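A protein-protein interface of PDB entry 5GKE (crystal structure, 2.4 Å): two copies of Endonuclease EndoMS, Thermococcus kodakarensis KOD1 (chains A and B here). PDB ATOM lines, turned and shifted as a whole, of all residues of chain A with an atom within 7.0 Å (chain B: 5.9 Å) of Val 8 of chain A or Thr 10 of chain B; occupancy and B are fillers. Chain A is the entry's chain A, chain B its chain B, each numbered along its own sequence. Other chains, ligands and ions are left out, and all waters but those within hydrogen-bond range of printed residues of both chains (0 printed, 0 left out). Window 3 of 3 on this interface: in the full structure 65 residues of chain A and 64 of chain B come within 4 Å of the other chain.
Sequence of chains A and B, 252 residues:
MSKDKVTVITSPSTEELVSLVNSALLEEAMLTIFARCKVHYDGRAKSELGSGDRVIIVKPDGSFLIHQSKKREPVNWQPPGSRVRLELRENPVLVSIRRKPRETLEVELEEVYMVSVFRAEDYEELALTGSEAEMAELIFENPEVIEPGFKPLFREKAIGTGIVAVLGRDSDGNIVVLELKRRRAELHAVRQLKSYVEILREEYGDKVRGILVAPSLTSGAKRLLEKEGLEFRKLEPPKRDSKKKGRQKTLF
The backbone carbonyl oxygen of Tyr 113 of chain B is in hydrogen-bond range of the backbone NH of Ser 11 of chain B (2.7 Å). The backbone NH (N) of Tyr 113 of chain B sits at hydrogen-bond distance from the backbone carbonyl oxygen (O) of Phe 34 of chain B (2.8 Å). The backbone carbonyl oxygen (O) of Met 114 of chain B is in hydrogen-bond range of the backbone NH (N) of Phe 34 of chain B (2.9 Å).
Among the printed residues, merely in contact across the chains: Ser 116 of chain A with Phe 34 of chain B, Val 6 of chain A with Tyr 113 of chain B, Thr 10 of chain A with Val 8 of chain B, Val 8 of chain A with Thr 10 of chain B, Val 6 of chain A with Phe 34 of chain B and Val 8 of chain A with Val 8 of chain B.
Of chain B, only Val 8 and Thr 10 come within 4 Å of Val 8 of chain A. Of chain A, only Val 8 comes within 4 Å of Thr 10 of chain B. Printed residues of chain B within 4 Å of Ser 116 of chain A: Phe 34. Of the printed residues of chain A, Val 8 of chain B touches Val 8 and Thr 10. Ser 11 of chain B touches none of the printed residues of chain A. The nearest residue of chain A that does not touch Thr 10 of chain B is Val 6 of chain A (4.1 Å). The nearest printed residue of chain A that does not touch Phe 34 of chain B is Val 117 of chain A (5.2 Å).
Of the 10 printed residues of chain A, 4 touch a printed residue of chain B. Hydrophobic or aromatic side chains of chain B within 4 Å of the printed part of chain A: Val 8, Phe 34 and Tyr 113. Among the printed residues, no Asp or Glu carboxylate lies within 4 Å of a Lys or Arg side-chain nitrogen of the other chain.
Val 8 of chain B touches its own counterpart, Val 8 of chain A. Val 8 of chain A touches Thr 10 of chain B, and with the chains exchanged Thr 10 of chain A touches Val 8 of chain B. 5 positions are printed for both chains. Of the 6 pairs that touch across the chains among the printed residues, 3 have their exchanged pair printed and touching as well.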
ATOM      1  N   VAL A   6     -16.006  23.424   0.026  1.00  0.00           N
ATOM      2  CA  VAL A   6     -14.984  22.715   0.796  1.00  0.00           C
ATOM      3  C   VAL A   6     -13.888  23.633   1.326  1.00  0.00           C
ATOM      4  O   VAL A   6     -13.402  24.500   0.627  1.00  0.00           O
ATOM      5  CB  VAL A   6     -14.307  21.587  -0.057  1.00  0.00           C
ATOM      6  CG1 VAL A   6     -13.156  20.905   0.705  1.00  0.00           C
ATOM      7  CG2 VAL A   6     -15.325  20.562  -0.492  1.00  0.00           C
ATOM      8  N   THR A   7     -13.488  23.404   2.569  1.00  0.00           N
ATOM      9  CA  THR A   7     -12.357  24.087   3.168  1.00  0.00           C
ATOM     10  C   THR A   7     -11.400  23.038   3.713  1.00  0.00           C
ATOM     11  O   THR A   7     -11.821  22.119   4.384  1.00  0.00           O
ATOM     12  CB  THR A   7     -12.805  25.018   4.307  1.00  0.00           C
ATOM     13  OG1 THR A   7     -13.985  25.728   3.922  1.00  0.00           O
ATOM     14  CG2 THR A   7     -11.720  25.989   4.653  1.00  0.00           C
ATOM     15  N   VAL A   8     -10.118  23.158   3.419  1.00  0.00           N
ATOM     16  CA  VAL A   8      -9.167  22.129   3.794  1.00  0.00           C
ATOM     17  C   VAL A   8      -7.970  22.789   4.408  1.00  0.00           C
ATOM     18  O   VAL A   8      -7.422  23.723   3.832  1.00  0.00           O
ATOM     19  CB  VAL A   8      -8.690  21.287   2.576  1.00  0.00           C
ATOM     20  CG1 VAL A   8      -7.616  20.302   3.000  1.00  0.00           C
ATOM     21  CG2 VAL A   8      -9.830  20.554   1.944  1.00  0.00           C
ATOM     22  N   ILE A   9      -7.556  22.319   5.571  1.00  0.00           N
ATOM     23  CA  ILE A   9      -6.284  22.748   6.125  1.00  0.00           C
ATOM     24  C   ILE A   9      -5.471  21.547   6.572  1.00  0.00           C
ATOM     25  O   ILE A   9      -5.944  20.719   7.343  1.00  0.00           O
ATOM     26  CB  ILE A   9      -6.464  23.679   7.320  1.00  0.00           C
ATOM     27  CG1 ILE A   9      -7.248  24.925   6.915  1.00  0.00           C
ATOM     28  CG2 ILE A   9      -5.109  24.070   7.893  1.00  0.00           C
ATOM     29  CD1 ILE A   9      -7.448  25.868   8.058  1.00  0.00           C
ATOM     30  N   THR A  10      -4.240  21.467   6.092  1.00  0.00           N
ATOM     31  CA  THR A  10      -3.326  20.422   6.508  1.00  0.00           C
ATOM     32  C   THR A  10      -2.470  20.930   7.647  1.00  0.00           C
ATOM     33  O   THR A  10      -2.184  22.125   7.730  1.00  0.00           O
ATOM     34  CB  THR A  10      -2.444  19.947   5.341  1.00  0.00           C
ATOM     35  OG1 THR A  10      -1.811  21.081   4.726  1.00  0.00           O
ATOM     36  CG2 THR A  10      -3.308  19.230   4.301  1.00  0.00           C
ATOM     37  N   LEU A  20     -12.321  25.701  12.261  1.00  0.00           N
ATOM     38  CA  LEU A  20     -13.014  24.841  11.291  1.00  0.00           C
ATOM     39  C   LEU A  20     -14.032  23.918  11.915  1.00  0.00           C
ATOM     40  O   LEU A  20     -15.131  23.753  11.386  1.00  0.00           O
ATOM     41  CB  LEU A  20     -12.019  24.004  10.510  1.00  0.00           C
ATOM     42  CG  LEU A  20     -11.410  24.769   9.331  1.00  0.00           C
ATOM     43  CD1 LEU A  20     -10.577  23.843   8.454  1.00  0.00           C
ATOM     44  CD2 LEU A  20     -12.521  25.387   8.533  1.00  0.00           C
ATOM     45  N   MET A 114      -5.067  16.578   8.901  1.00  0.00           N
ATOM     46  CA  MET A 114      -5.946  17.381   8.071  1.00  0.00           C
ATOM     47  C   MET A 114      -7.267  17.618   8.787  1.00  0.00           C
ATOM     48  O   MET A 114      -7.731  16.764   9.544  1.00  0.00           O
ATOM     49  CB  MET A 114      -6.180  16.699   6.718  1.00  0.00           C
ATOM     50  CG  MET A 114      -6.881  17.584   5.702  1.00  0.00           C
ATOM     51  SD  MET A 114      -7.599  16.644   4.341  1.00  0.00           S
ATOM     52  CE  MET A 114      -9.169  16.193   5.104  1.00  0.00           C
ATOM     53  N   VAL A 115      -7.856  18.782   8.551  1.00  0.00           N
ATOM     54  CA  VAL A 115      -9.224  19.056   8.958  1.00  0.00           C
ATOM     55  C   VAL A 115      -9.939  19.667   7.764  1.00  0.00           C
ATOM     56  O   VAL A 115      -9.356  20.432   7.006  1.00  0.00           O
ATOM     57  CB  VAL A 115      -9.294  19.997  10.188  1.00  0.00           C
ATOM     58  CG1 VAL A 115      -8.468  21.248   9.964  1.00  0.00           C
ATOM     59  CG2 VAL A 115     -10.727  20.367  10.491  1.00  0.00           C
ATOM     60  N   SER A 116     -11.200  19.320   7.579  1.00  0.00           N
ATOM     61  CA  SER A 116     -11.926  19.800   6.418  1.00  0.00           C
ATOM     62  C   SER A 116     -13.386  20.021   6.729  1.00  0.00           C
ATOM     63  O   SER A 116     -13.993  19.311   7.546  1.00  0.00           O
ATOM     64  CB  SER A 116     -11.797  18.817   5.250  1.00  0.00           C
ATOM     65  OG  SER A 116     -12.478  17.603   5.548  1.00  0.00           O
ATOM     66  N   VAL A 117     -13.946  21.015   6.061  1.00  0.00           N
ATOM     67  CA  VAL A 117     -15.348  21.324   6.204  1.00  0.00           C
ATOM     68  C   VAL A 117     -15.986  21.163   4.849  1.00  0.00           C
ATOM     69  O   VAL A 117     -15.556  21.775   3.871  1.00  0.00           O
ATOM     70  CB  VAL A 117     -15.566  22.744   6.748  1.00  0.00           C
ATOM     71  CG1 VAL A 117     -17.027  23.129   6.675  1.00  0.00           C
ATOM     72  CG2 VAL A 117     -15.060  22.834   8.166  1.00  0.00           C
ATOM     73  N   VAL B   8      -3.685  16.094  -0.711  1.00  0.00           N
ATOM     74  CA  VAL B   8      -5.045  16.513  -0.951  1.00  0.00           C
ATOM     75  C   VAL B   8      -5.083  17.593  -2.007  1.00  0.00           C
ATOM     76  O   VAL B   8      -4.270  18.503  -1.997  1.00  0.00           O
ATOM     77  CB  VAL B   8      -5.729  17.019   0.367  1.00  0.00           C
ATOM     78  CG1 VAL B   8      -4.773  17.849   1.190  1.00  0.00           C
ATOM     79  CG2 VAL B   8      -6.987  17.808   0.053  1.00  0.00           C
ATOM     80  N   ILE B   9      -6.036  17.470  -2.916  1.00  0.00           N
ATOM     81  CA  ILE B   9      -6.247  18.438  -3.961  1.00  0.00           C
ATOM     82  C   ILE B   9      -7.715  18.811  -3.971  1.00  0.00           C
ATOM     83  O   ILE B   9      -8.567  17.934  -4.093  1.00  0.00           O
ATOM     84  CB  ILE B   9      -5.846  17.876  -5.349  1.00  0.00           C
ATOM     85  CG1 ILE B   9      -4.345  17.614  -5.397  1.00  0.00           C
ATOM     86  CG2 ILE B   9      -6.284  18.807  -6.475  1.00  0.00           C
ATOM     87  CD1 ILE B   9      -3.889  16.971  -6.687  1.00  0.00           C
ATOM     88  N   THR B  10      -8.029  20.090  -3.781  1.00  0.00           N
ATOM     89  CA  THR B  10      -9.391  20.545  -4.019  1.00  0.00           C
ATOM     90  C   THR B  10      -9.554  20.832  -5.499  1.00  0.00           C
ATOM     91  O   THR B  10      -8.573  21.072  -6.185  1.00  0.00           O
ATOM     92  CB  THR B  10      -9.745  21.766  -3.174  1.00  0.00           C
ATOM     93  OG1 THR B  10      -8.690  22.724  -3.262  1.00  0.00           O
ATOM     94  CG2 THR B  10      -9.897  21.335  -1.717  1.00  0.00           C
ATOM     95  N   SER B  11     -10.790  20.776  -5.973  1.00  0.00           N
ATOM     96  CA  SER B  11     -11.128  20.978  -7.379  1.00  0.00           C
ATOM     97  C   SER B  11     -10.112  20.387  -8.349  1.00  0.00           C
ATOM     98  O   SER B  11      -9.584  21.094  -9.214  1.00  0.00           O
ATOM     99  CB  SER B  11     -11.303  22.458  -7.659  1.00  0.00           C
ATOM    100  OG  SER B  11     -12.622  22.866  -7.357  1.00  0.00           O
ATOM    101  N   PRO B  12      -9.845  19.080  -8.217  1.00  0.00           N
ATOM    102  CA  PRO B  12      -8.832  18.429  -9.050  1.00  0.00           C
ATOM    103  C   PRO B  12      -9.259  18.293 -10.510  1.00  0.00           C
ATOM    104  O   PRO B  12     -10.450  18.196 -10.835  1.00  0.00           O
ATOM    105  CB  PRO B  12      -8.701  17.049  -8.409  1.00  0.00           C
ATOM    106  CG  PRO B  12     -10.080  16.774  -7.938  1.00  0.00           C
ATOM    107  CD  PRO B  12     -10.591  18.093  -7.411  1.00  0.00           C
ATOM    108  N   GLU B  16      -5.430  14.860 -12.265  1.00  0.00           N
ATOM    109  CA  GLU B  16      -5.058  14.956 -10.869  1.00  0.00           C
ATOM    110  C   GLU B  16      -5.813  13.880 -10.104  1.00  0.00           C
ATOM    111  O   GLU B  16      -5.219  13.143  -9.312  1.00  0.00           O
ATOM    112  CB  GLU B  16      -5.338  16.354 -10.335  1.00  0.00           C
ATOM    113  CG  GLU B  16      -4.158  17.285 -10.567  1.00  0.00           C
ATOM    114  CD  GLU B  16      -4.412  18.703 -10.111  1.00  0.00           C
ATOM    115  OE1 GLU B  16      -5.515  19.234 -10.388  1.00  0.00           O
ATOM    116  OE2 GLU B  16      -3.496  19.279  -9.478  1.00  0.00           O
ATOM    117  N   PHE B  34     -14.645  14.163  -1.692  1.00  0.00           N
ATOM    118  CA  PHE B  34     -15.925  14.839  -1.584  1.00  0.00           C
ATOM    119  C   PHE B  34     -16.383  15.122  -3.002  1.00  0.00           C
ATOM    120  O   PHE B  34     -15.642  15.706  -3.799  1.00  0.00           O
ATOM    121  CB  PHE B  34     -15.852  16.145  -0.770  1.00  0.00           C
ATOM    122  CG  PHE B  34     -15.202  16.022   0.593  1.00  0.00           C
ATOM    123  CD1 PHE B  34     -14.583  17.135   1.166  1.00  0.00           C
ATOM    124  CD2 PHE B  34     -15.233  14.834   1.319  1.00  0.00           C
ATOM    125  CE1 PHE B  34     -13.976  17.060   2.414  1.00  0.00           C
ATOM    126  CE2 PHE B  34     -14.627  14.750   2.586  1.00  0.00           C
ATOM    127  CZ  PHE B  34     -14.007  15.854   3.134  1.00  0.00           C
ATOM    128  N   VAL B 112     -15.876  16.526  -8.599  1.00  0.00           N
ATOM    129  CA  VAL B 112     -15.050  16.214  -7.454  1.00  0.00           C
ATOM    130  C   VAL B 112     -14.600  17.506  -6.795  1.00  0.00           C
ATOM    131  O   VAL B 112     -13.875  18.300  -7.383  1.00  0.00           O
ATOM    132  CB  VAL B 112     -13.838  15.364  -7.848  1.00  0.00           C
ATOM    133  CG1 VAL B 112     -12.995  15.047  -6.638  1.00  0.00           C
ATOM    134  CG2 VAL B 112     -14.311  14.083  -8.515  1.00  0.00           C
ATOM    135  N   TYR B 113     -15.058  17.735  -5.575  1.00  0.00           N
ATOM    136  CA  TYR B 113     -14.639  18.923  -4.860  1.00  0.00           C
ATOM    137  C   TYR B 113     -13.270  18.716  -4.233  1.00  0.00           C
ATOM    138  O   TYR B 113     -12.478  19.646  -4.132  1.00  0.00           O
ATOM    139  CB  TYR B 113     -15.649  19.283  -3.788  1.00  0.00           C
ATOM    140  CG  TYR B 113     -17.071  19.350  -4.273  1.00  0.00           C
ATOM    141  CD1 TYR B 113     -17.458  20.282  -5.232  1.00  0.00           C
ATOM    142  CD2 TYR B 113     -18.044  18.500  -3.744  1.00  0.00           C
ATOM    143  CE1 TYR B 113     -18.777  20.351  -5.674  1.00  0.00           C
ATOM    144  CE2 TYR B 113     -19.365  18.574  -4.158  1.00  0.00           C
ATOM    145  CZ  TYR B 113     -19.725  19.499  -5.125  1.00  0.00           C
ATOM    146  OH  TYR B 113     -21.032  19.573  -5.535  1.00  0.00           O
ATOM    147  N   MET B 114     -13.011  17.499  -3.768  1.00  0.00           N
ATOM    148  CA  MET B 114     -11.757  17.211  -3.094  1.00  0.00           C
ATOM    149  C   MET B 114     -11.396  15.748  -3.241  1.00  0.00           C
ATOM    150  O   MET B 114     -12.269  14.889  -3.156  1.00  0.00           O
ATOM    151  CB  MET B 114     -11.854  17.574  -1.602  1.00  0.00           C
ATOM    152  CG  MET B 114     -10.510  17.566  -0.898  1.00  0.00           C
ATOM    153  SD  MET B 114     -10.435  16.589   0.593  1.00  0.00           S
ATOM    154  CE  MET B 114     -10.869  15.008  -0.044  1.00  0.00           C
ATOM    155  N   VAL B 115     -10.113  15.460  -3.422  1.00  0.00           N
ATOM    156  CA  VAL B 115      -9.630  14.084  -3.376  1.00  0.00           C
ATOM    157  C   VAL B 115      -8.402  14.075  -2.509  1.00  0.00           C
ATOM    158  O   VAL B 115      -7.634  15.037  -2.506  1.00  0.00           O
ATOM    159  CB  VAL B 115      -9.292  13.499  -4.780  1.00  0.00           C
ATOM    160  CG1 VAL B 115      -8.424  14.462  -5.567  1.00  0.00           C
ATOM    161  CG2 VAL B 115      -8.600  12.133  -4.647  1.00  0.00           C
